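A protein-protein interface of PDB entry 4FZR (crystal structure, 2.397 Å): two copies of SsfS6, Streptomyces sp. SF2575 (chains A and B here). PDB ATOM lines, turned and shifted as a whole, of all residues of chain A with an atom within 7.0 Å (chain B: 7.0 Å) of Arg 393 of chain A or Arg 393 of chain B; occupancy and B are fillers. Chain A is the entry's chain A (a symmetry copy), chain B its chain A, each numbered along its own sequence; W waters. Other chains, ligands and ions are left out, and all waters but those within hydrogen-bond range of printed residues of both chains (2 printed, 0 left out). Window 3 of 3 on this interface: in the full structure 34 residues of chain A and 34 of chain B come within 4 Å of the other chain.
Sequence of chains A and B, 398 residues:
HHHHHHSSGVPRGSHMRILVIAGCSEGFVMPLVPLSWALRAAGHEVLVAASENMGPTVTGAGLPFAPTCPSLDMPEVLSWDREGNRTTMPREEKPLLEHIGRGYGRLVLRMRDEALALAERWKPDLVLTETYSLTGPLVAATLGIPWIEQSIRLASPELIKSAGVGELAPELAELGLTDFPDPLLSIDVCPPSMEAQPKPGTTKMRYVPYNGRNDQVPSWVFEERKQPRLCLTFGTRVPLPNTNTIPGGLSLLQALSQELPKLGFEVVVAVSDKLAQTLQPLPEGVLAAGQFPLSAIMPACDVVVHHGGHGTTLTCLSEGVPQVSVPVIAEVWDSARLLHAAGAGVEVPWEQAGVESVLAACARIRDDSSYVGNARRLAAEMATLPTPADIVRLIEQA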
ATOM      1  N   LEU A  39     -16.331   9.078  11.924  1.00  0.00           N
ATOM      2  CA  LEU A  39     -16.753   8.365  13.123  1.00  0.00           C
ATOM      3  C   LEU A  39     -17.196   9.349  14.196  1.00  0.00           C
ATOM      4  O   LEU A  39     -18.263   9.201  14.793  1.00  0.00           O
ATOM      5  CB  LEU A  39     -15.611   7.495  13.654  1.00  0.00           C
ATOM      6  CG  LEU A  39     -15.190   6.328  12.756  1.00  0.00           C
ATOM      7  CD1 LEU A  39     -13.917   5.663  13.276  1.00  0.00           C
ATOM      8  CD2 LEU A  39     -16.319   5.313  12.629  1.00  0.00           C
ATOM      9  N   ALA A  42     -20.407  10.892  13.660  1.00  0.00           N
ATOM     10  CA  ALA A  42     -21.501   9.963  13.918  1.00  0.00           C
ATOM     11  C   ALA A  42     -21.631   9.657  15.408  1.00  0.00           C
ATOM     12  O   ALA A  42     -22.213   8.643  15.791  1.00  0.00           O
ATOM     13  CB  ALA A  42     -21.296   8.678  13.133  1.00  0.00           C
ATOM     14  N   HIS A  44     -19.430   8.887  17.697  1.00  0.00           N
ATOM     15  CA  HIS A  44     -18.514   7.936  18.321  1.00  0.00           C
ATOM     16  C   HIS A  44     -17.317   8.641  18.957  1.00  0.00           C
ATOM     17  O   HIS A  44     -17.049   9.808  18.678  1.00  0.00           O
ATOM     18  CB  HIS A  44     -18.060   6.894  17.296  1.00  0.00           C
ATOM     19  CG  HIS A  44     -19.197   6.249  16.566  1.00  0.00           C
ATOM     20  ND1 HIS A  44     -20.156   5.492  17.202  1.00  0.00           N
ATOM     21  CD2 HIS A  44     -19.541   6.269  15.256  1.00  0.00           C
ATOM     22  CE1 HIS A  44     -21.037   5.063  16.315  1.00  0.00           C
ATOM     23  NE2 HIS A  44     -20.686   5.520  15.127  1.00  0.00           N
ATOM     24  N   THR A 387     -18.938   7.185   0.430  1.00  0.00           N
ATOM     25  CA  THR A 387     -18.146   8.140   1.197  1.00  0.00           C
ATOM     26  C   THR A 387     -17.750   7.541   2.542  1.00  0.00           C
ATOM     27  O   THR A 387     -18.316   6.532   2.964  1.00  0.00           O
ATOM     28  CB  THR A 387     -18.937   9.426   1.470  1.00  0.00           C
ATOM     29  OG1 THR A 387     -19.989   9.153   2.409  1.00  0.00           O
ATOM     30  CG2 THR A 387     -19.525   9.973   0.181  1.00  0.00           C
ATOM     31  N   PRO A 388     -16.764   8.153   3.217  1.00  0.00           N
ATOM     32  CA  PRO A 388     -16.419   7.763   4.589  1.00  0.00           C
ATOM     33  C   PRO A 388     -17.628   7.748   5.528  1.00  0.00           C
ATOM     34  O   PRO A 388     -17.701   6.899   6.415  1.00  0.00           O
ATOM     35  CB  PRO A 388     -15.412   8.836   5.004  1.00  0.00           C
ATOM     36  CG  PRO A 388     -14.717   9.172   3.721  1.00  0.00           C
ATOM     37  CD  PRO A 388     -15.786   9.105   2.657  1.00  0.00           C
ATOM     38  N   ALA A 389     -18.567   8.668   5.333  1.00  0.00           N
ATOM     39  CA  ALA A 389     -19.793   8.673   6.127  1.00  0.00           C
ATOM     40  C   ALA A 389     -20.602   7.400   5.865  1.00  0.00           C
ATOM     41  O   ALA A 389     -21.169   6.814   6.791  1.00  0.00           O
ATOM     42  CB  ALA A 389     -20.629   9.910   5.817  1.00  0.00           C
ATOM     43  N   ASP A 390     -20.642   6.973   4.602  1.00  0.00           N
ATOM     44  CA  ASP A 390     -21.336   5.740   4.225  1.00  0.00           C
ATOM     45  C   ASP A 390     -20.695   4.544   4.932  1.00  0.00           C
ATOM     46  O   ASP A 390     -21.388   3.684   5.477  1.00  0.00           O
ATOM     47  CB  ASP A 390     -21.297   5.507   2.704  1.00  0.00           C
ATOM     48  CG  ASP A 390     -22.042   6.578   1.907  1.00  0.00           C
ATOM     49  OD1 ASP A 390     -23.010   7.169   2.427  1.00  0.00           O
ATOM     50  OD2 ASP A 390     -21.662   6.816   0.739  1.00  0.00           O
ATOM     51  N   ILE A 391     -19.365   4.497   4.919  1.00  0.00           N
ATOM     52  CA  ILE A 391     -18.618   3.393   5.524  1.00  0.00           C
ATOM     53  C   ILE A 391     -18.845   3.279   7.032  1.00  0.00           C
ATOM     54  O   ILE A 391     -18.829   2.180   7.587  1.00  0.00           O
ATOM     55  CB  ILE A 391     -17.105   3.528   5.257  1.00  0.00           C
ATOM     56  CG1 ILE A 391     -16.804   3.270   3.775  1.00  0.00           C
ATOM     57  CG2 ILE A 391     -16.304   2.576   6.157  1.00  0.00           C
ATOM     58  CD1 ILE A 391     -17.301   1.941   3.258  1.00  0.00           C
ATOM     59  N   VAL A 392     -19.052   4.411   7.694  1.00  0.00           N
ATOM     60  CA  VAL A 392     -19.311   4.397   9.126  1.00  0.00           C
ATOM     61  C   VAL A 392     -20.608   3.646   9.415  1.00  0.00           C
ATOM     62  O   VAL A 392     -20.693   2.883  10.377  1.00  0.00           O
ATOM     63  CB  VAL A 392     -19.381   5.822   9.719  1.00  0.00           C
ATOM     64  CG1 VAL A 392     -19.873   5.777  11.158  1.00  0.00           C
ATOM     65  CG2 VAL A 392     -18.017   6.499   9.649  1.00  0.00           C
ATOM     66  N   ARG A 393     -21.616   3.850   8.571  1.00  0.00           N
ATOM     67  CA  ARG A 393     -22.883   3.144   8.722  1.00  0.00           C
ATOM     68  C   ARG A 393     -22.670   1.641   8.582  1.00  0.00           C
ATOM     69  O   ARG A 393     -23.245   0.850   9.326  1.00  0.00           O
ATOM     70  CB  ARG A 393     -23.903   3.641   7.700  1.00  0.00           C
ATOM     71  CG  ARG A 393     -24.351   5.062   7.962  1.00  0.00           C
ATOM     72  CD  ARG A 393     -25.301   5.564   6.906  1.00  0.00           C
ATOM     73  NE  ARG A 393     -24.940   6.919   6.480  1.00  0.00           N
ATOM     74  CZ  ARG A 393     -24.604   7.260   5.236  1.00  0.00           C
ATOM     75  NH1 ARG A 393     -24.559   6.363   4.256  1.00  0.00           N
ATOM     76  NH2 ARG A 393     -24.293   8.518   4.964  1.00  0.00           N
ATOM     77  N   LEU A 394     -21.833   1.254   7.627  1.00  0.00           N
ATOM     78  CA  LEU A 394     -21.455  -0.145   7.474  1.00  0.00           C
ATOM     79  C   LEU A 394     -20.828  -0.658   8.766  1.00  0.00           C
ATOM     80  O   LEU A 394     -21.248  -1.682   9.306  1.00  0.00           O
ATOM     81  CB  LEU A 394     -20.473  -0.317   6.311  1.00  0.00           C
ATOM     82  CG  LEU A 394     -21.069  -0.657   4.944  1.00  0.00           C
ATOM     83  CD1 LEU A 394     -22.151   0.334   4.543  1.00  0.00           C
ATOM     84  CD2 LEU A 394     -19.971  -0.701   3.894  1.00  0.00           C
ATOM     85  N   ILE A 395     -19.831   0.070   9.262  1.00  0.00           N
ATOM     86  CA  ILE A 395     -19.089  -0.339  10.448  1.00  0.00           C
ATOM     87  C   ILE A 395     -20.011  -0.590  11.634  1.00  0.00           C
ATOM     88  O   ILE A 395     -19.850  -1.571  12.359  1.00  0.00           O
ATOM     89  CB  ILE A 395     -18.053   0.730  10.850  1.00  0.00           C
ATOM     90  CG1 ILE A 395     -16.882   0.730   9.865  1.00  0.00           C
ATOM     91  CG2 ILE A 395     -17.545   0.485  12.272  1.00  0.00           C
ATOM     92  CD1 ILE A 395     -15.913   1.875  10.072  1.00  0.00           C
ATOM     93  N   GLU A 396     -20.982   0.296  11.822  1.00  0.00           N
ATOM     94  CA  GLU A 396     -21.853   0.231  12.993  1.00  0.00           C
ATOM     95  C   GLU A 396     -22.963  -0.818  12.867  1.00  0.00           C
ATOM     96  O   GLU A 396     -23.854  -0.888  13.715  1.00  0.00           O
ATOM     97  CB  GLU A 396     -22.437   1.616  13.319  1.00  0.00           C
ATOM     98  CG  GLU A 396     -23.235   2.273  12.200  1.00  0.00           C
ATOM     99  CD  GLU A 396     -23.432   3.771  12.415  1.00  0.00           C
ATOM    100  OE1 GLU A 396     -22.817   4.329  13.350  1.00  0.00           O
ATOM    101  OE2 GLU A 396     -24.200   4.390  11.646  1.00  0.00           O
ATOM    102  N   GLN A 397     -22.902  -1.636  11.818  1.00  0.00           N
ATOM    103  CA  GLN A 397     -23.816  -2.769  11.666  1.00  0.00           C
ATOM    104  C   GLN A 397     -23.046  -4.081  11.562  1.00  0.00           C
ATOM    105  O   GLN A 397     -21.944  -4.124  11.014  1.00  0.00           O
ATOM    106  CB  GLN A 397     -24.697  -2.590  10.429  1.00  0.00           C
ATOM    107  CG  GLN A 397     -25.693  -1.452  10.533  1.00  0.00           C
ATOM    108  CD  GLN A 397     -26.447  -1.234   9.237  1.00  0.00           C
ATOM    109  OE1 GLN A 397     -25.934  -1.514   8.153  1.00  0.00           O
ATOM    110  NE2 GLN A 397     -27.675  -0.739   9.341  1.00  0.00           N
ATOM    111  N   LEU B  39     -19.982  17.082   7.029  1.00  0.00           N
ATOM    112  CA  LEU B  39     -20.209  17.369   5.619  1.00  0.00           C
ATOM    113  C   LEU B  39     -19.046  16.856   4.781  1.00  0.00           C
ATOM    114  O   LEU B  39     -19.241  16.177   3.772  1.00  0.00           O
ATOM    115  CB  LEU B  39     -20.381  18.875   5.404  1.00  0.00           C
ATOM    116  CG  LEU B  39     -21.631  19.497   6.032  1.00  0.00           C
ATOM    117  CD1 LEU B  39     -21.594  21.022   5.939  1.00  0.00           C
ATOM    118  CD2 LEU B  39     -22.893  18.945   5.379  1.00  0.00           C
ATOM    119  N   ALA B  42     -18.926  13.287   4.308  1.00  0.00           N
ATOM    120  CA  ALA B  42     -19.939  12.834   3.362  1.00  0.00           C
ATOM    121  C   ALA B  42     -19.607  13.273   1.939  1.00  0.00           C
ATOM    122  O   ALA B  42     -20.486  13.329   1.079  1.00  0.00           O
ATOM    123  CB  ALA B  42     -21.307  13.356   3.768  1.00  0.00           C
ATOM    124  N   HIS B  44     -18.628  16.127   0.687  1.00  0.00           N
ATOM    125  CA  HIS B  44     -18.899  17.502   0.274  1.00  0.00           C
ATOM    126  C   HIS B  44     -17.665  18.391   0.431  1.00  0.00           C
ATOM    127  O   HIS B  44     -16.706  18.028   1.110  1.00  0.00           O
ATOM    128  CB  HIS B  44     -20.086  18.063   1.059  1.00  0.00           C
ATOM    129  CG  HIS B  44     -21.290  17.173   1.026  1.00  0.00           C
ATOM    130  ND1 HIS B  44     -21.956  16.865  -0.140  1.00  0.00           N
ATOM    131  CD2 HIS B  44     -21.933  16.506   2.014  1.00  0.00           C
ATOM    132  CE1 HIS B  44     -22.963  16.055   0.131  1.00  0.00           C
ATOM    133  NE2 HIS B  44     -22.973  15.823   1.430  1.00  0.00           N
ATOM    134  N   THR B 387     -27.267  12.488  15.296  1.00  0.00           N
ATOM    135  CA  THR B 387     -25.886  12.957  15.238  1.00  0.00           C
ATOM    136  C   THR B 387     -25.707  13.934  14.081  1.00  0.00           C
ATOM    137  O   THR B 387     -26.560  14.013  13.195  1.00  0.00           O
ATOM    138  CB  THR B 387     -24.911  11.792  15.025  1.00  0.00           C
ATOM    139  OG1 THR B 387     -25.063  11.276  13.694  1.00  0.00           O
ATOM    140  CG2 THR B 387     -25.169  10.690  16.038  1.00  0.00           C
ATOM    141  N   PRO B 388     -24.600  14.694  14.089  1.00  0.00           N
ATOM    142  CA  PRO B 388     -24.246  15.542  12.944  1.00  0.00           C
ATOM    143  C   PRO B 388     -24.226  14.778  11.618  1.00  0.00           C
ATOM    144  O   PRO B 388     -24.595  15.338  10.586  1.00  0.00           O
ATOM    145  CB  PRO B 388     -22.851  16.044  13.314  1.00  0.00           C
ATOM    146  CG  PRO B 388     -22.898  16.133  14.808  1.00  0.00           C
ATOM    147  CD  PRO B 388     -23.730  14.954  15.251  1.00  0.00           C
ATOM    148  N   ALA B 389     -23.805  13.518  11.643  1.00  0.00           N
ATOM    149  CA  ALA B 389     -23.834  12.690  10.440  1.00  0.00           C
ATOM    150  C   ALA B 389     -25.276  12.487   9.967  1.00  0.00           C
ATOM    151  O   ALA B 389     -25.554  12.519   8.766  1.00  0.00           O
ATOM    152  CB  ALA B 389     -23.163  11.346  10.697  1.00  0.00           C
ATOM    153  N   ASP B 390     -26.189  12.289  10.919  1.00  0.00           N
ATOM    154  CA  ASP B 390     -27.611  12.135  10.606  1.00  0.00           C
ATOM    155  C   ASP B 390     -28.137  13.406   9.936  1.00  0.00           C
ATOM    156  O   ASP B 390     -28.850  13.344   8.933  1.00  0.00           O
ATOM    157  CB  ASP B 390     -28.444  11.846  11.869  1.00  0.00           C
ATOM    158  CG  ASP B 390     -28.094  10.518  12.537  1.00  0.00           C
ATOM    159  OD1 ASP B 390     -27.660   9.576  11.842  1.00  0.00           O
ATOM    160  OD2 ASP B 390     -28.272  10.411  13.770  1.00  0.00           O
ATOM    161  N   ILE B 391     -27.783  14.558  10.499  1.00  0.00           N
ATOM    162  CA  ILE B 391     -28.243  15.850   9.988  1.00  0.00           C
ATOM    163  C   ILE B 391     -27.768  16.126   8.562  1.00  0.00           C
ATOM    164  O   ILE B 391     -28.465  16.779   7.784  1.00  0.00           O
ATOM    165  CB  ILE B 391     -27.784  17.008  10.899  1.00  0.00           C
ATOM    166  CG1 ILE B 391     -28.543  16.966  12.231  1.00  0.00           C
ATOM    167  CG2 ILE B 391     -27.973  18.360  10.198  1.00  0.00           C
ATOM    168  CD1 ILE B 391     -30.047  16.982  12.095  1.00  0.00           C
ATOM    169  N   VAL B 392     -26.583  15.635   8.218  1.00  0.00           N
ATOM    170  CA  VAL B 392     -26.065  15.820   6.870  1.00  0.00           C
ATOM    171  C   VAL B 392     -26.975  15.123   5.861  1.00  0.00           C
ATOM    172  O   VAL B 392     -27.243  15.655   4.784  1.00  0.00           O
ATOM    173  CB  VAL B 392     -24.617  15.297   6.727  1.00  0.00           C
ATOM    174  CG1 VAL B 392     -24.194  15.298   5.266  1.00  0.00           C
ATOM    175  CG2 VAL B 392     -23.658  16.144   7.556  1.00  0.00           C
ATOM    176  N   ARG B 393     -27.463  13.938   6.217  1.00  0.00           N
ATOM    177  CA  ARG B 393     -28.384  13.209   5.352  1.00  0.00           C
ATOM    178  C   ARG B 393     -29.662  14.014   5.145  1.00  0.00           C
ATOM    179  O   ARG B 393     -30.195  14.079   4.039  1.00  0.00           O
ATOM    180  CB  ARG B 393     -28.701  11.836   5.938  1.00  0.00           C
ATOM    181  CG  ARG B 393     -27.512  10.901   5.917  1.00  0.00           C
ATOM    182  CD  ARG B 393     -27.819   9.574   6.564  1.00  0.00           C
ATOM    183  NE  ARG B 393     -26.734   9.167   7.462  1.00  0.00           N
ATOM    184  CZ  ARG B 393     -26.870   8.957   8.770  1.00  0.00           C
ATOM    185  NH1 ARG B 393     -28.038   9.118   9.384  1.00  0.00           N
ATOM    186  NH2 ARG B 393     -25.819   8.592   9.487  1.00  0.00           N
ATOM    187  N   LEU B 394     -30.145  14.633   6.215  1.00  0.00           N
ATOM    188  CA  LEU B 394     -31.290  15.529   6.118  1.00  0.00           C
ATOM    189  C   LEU B 394     -30.991  16.650   5.128  1.00  0.00           C
ATOM    190  O   LEU B 394     -31.762  16.893   4.199  1.00  0.00           O
ATOM    191  CB  LEU B 394     -31.635  16.119   7.489  1.00  0.00           C
ATOM    192  CG  LEU B 394     -32.686  15.379   8.319  1.00  0.00           C
ATOM    193  CD1 LEU B 394     -32.336  13.908   8.481  1.00  0.00           C
ATOM    194  CD2 LEU B 394     -32.837  16.044   9.678  1.00  0.00           C
ATOM    195  N   ILE B 395     -29.858  17.319   5.328  1.00  0.00           N
ATOM    196  CA  ILE B 395     -29.479  18.462   4.507  1.00  0.00           C
ATOM    197  C   ILE B 395     -29.468  18.116   3.024  1.00  0.00           C
ATOM    198  O   ILE B 395     -29.948  18.887   2.194  1.00  0.00           O
ATOM    199  CB  ILE B 395     -28.083  18.988   4.899  1.00  0.00           C
ATOM    200  CG1 ILE B 395     -28.148  19.713   6.244  1.00  0.00           C
ATOM    201  CG2 ILE B 395     -27.536  19.925   3.821  1.00  0.00           C
ATOM    202  CD1 ILE B 395     -26.790  20.093   6.797  1.00  0.00           C
ATOM    203  N   GLU B 396     -28.924  16.949   2.696  1.00  0.00           N
ATOM    204  CA  GLU B 396     -28.745  16.561   1.300  1.00  0.00           C
ATOM    205  C   GLU B 396     -30.030  16.040   0.644  1.00  0.00           C
ATOM    206  O   GLU B 396     -29.998  15.547  -0.485  1.00  0.00           O
ATOM    207  CB  GLU B 396     -27.601  15.543   1.156  1.00  0.00           C
ATOM    208  CG  GLU B 396     -27.756  14.261   1.964  1.00  0.00           C
ATOM    209  CD  GLU B 396     -26.446  13.494   2.112  1.00  0.00           C
ATOM    210  OE1 GLU B 396     -25.386  14.033   1.724  1.00  0.00           O
ATOM    211  OE2 GLU B 396     -26.476  12.351   2.621  1.00  0.00           O
ATOM    212  N   GLN B 397     -31.155  16.160   1.346  1.00  0.00           N
ATOM    213  CA  GLN B 397     -32.461  15.837   0.773  1.00  0.00           C
ATOM    214  C   GLN B 397     -33.394  17.042   0.824  1.00  0.00           C
ATOM    215  O   GLN B 397     -33.331  17.850   1.753  1.00  0.00           O
ATOM    216  CB  GLN B 397     -33.100  14.662   1.514  1.00  0.00           C
ATOM    217  CG  GLN B 397     -32.386  13.339   1.319  1.00  0.00           C
ATOM    218  CD  GLN B 397     -32.977  12.238   2.176  1.00  0.00           C
ATOM    219  OE1 GLN B 397     -33.522  12.498   3.250  1.00  0.00           O
ATOM    220  NE2 GLN B 397     -32.881  11.001   1.702  1.00  0.00           N
HETATM  221  O   HOH W   1     -23.746   7.269  11.177  1.00  0.00           O
HETATM  222  O   HOH W   2     -24.081  11.341   4.020  1.00  0.00           O
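Ala 42 of chain A touches Thr 387 of chain B, and with the chains exchanged Thr 387 of chain A touches Ala 42 of chain B. Ala 42 of chain A touches Ala 389 of chain B, and with the chains exchanged Ala 389 of chain A touches Ala 42 of chain B. Arg 393 of chain B touches its own counterpart, Arg 393 of chain A. 14 positions are printed for both chains. Of the 5 pairs that touch across the chains among the printed residues, 5 have their exchanged pair printed and touching as well.
Among the printed residues, pairs that only touch across the chains: Ala 42 of chain A with Thr 387 of chain B (3.6 Å), Ala 42 of chain A with Ala 389 of chain B (3.9 Å), Thr 387 of chain A with Ala 42 of chain B (3.6 Å) and Ala 389 of chain A with Ala 42 of chain B (3.9 Å).
Printed residues of chain B within 4 Å of Ala 42 of chain A: Thr 387 and Ala 389. Of the printed residues of chain B, Thr 387 of chain A touches Ala 42. Printed residues of chain B within 4 Å of Ala 389 of chain A: Ala 42 (3.9 Å). Of chain B, only Arg 393 (3.0 Å) comes within 4 Å of Arg 393 of chain A. Leu 394 of chain A touches none of the printed residues of chain B. Of the printed residues of chain A, Ala 42 of chain B touches Thr 387 and Ala 389. Printed residues of chain A within 4 Å of Ala 389 of chain B: Ala 42. Ile 391 of chain B touches none of the printed residues of chain A. Arg 393 of chain B touches just one residue of chain A: Arg 393. The nearest residue of chain B that does not touch Arg 393 of chain A is Glu 396 of chain B (5.0 Å). The nearest printed residue of chain B that does not touch Thr 387 of chain A is His 44 of chain B (6.2 Å).
Water W1 lies within hydrogen-bond range of the side-chain carboxylate (OE2) of Glu 396 of chain A and the guanidinium group (NH2) of Arg 393 of chain B. Water W2 bridges OE2 of Glu 396 of chain B (3.0 Å) and NH2 of Arg 393 of chain A (3.0 Å).
Along chain A the printed residues that touch a printed residue of chain B span positions 42 to 393. Of the 14 printed residues of chain B, 4 touch a printed residue of chain A. Among the printed residues, 5 pairs touch across the chains. Among the printed residues, no Asp or Glu carboxylate lies within 4 Å of a Lys or Arg side-chain nitrogen of the other chain.
The side-chain hydroxyl (OG1) of Thr 387 of chain B lies close to the backbone NH (N) of Ala 389 of chain B (3.3 Å). N of Thr 387 of chain B sits at hydrogen-bond distance from OD2 of Asp 390 of chain B (2.8 Å). OD1 of Asp 390 of chain B lies within salt-bridge range of NH1 of Arg 393 of chain B. OG1 of Thr 387 of chain A sits close to N of Ala 389 of chain A (3.3 Å). OD2 of Asp 390 of chain A sits at hydrogen-bond distance from N of Thr 387 of chain A. The side-chain carboxylate (OD1) of Asp 390 of chain A lies within salt-bridge range of the guanidinium group (NH1) of Arg 393 of chain A (2.5 Å).
NE of Arg 393 of chain A sits close to NE of Arg 393 of chain B (3.0 Å).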
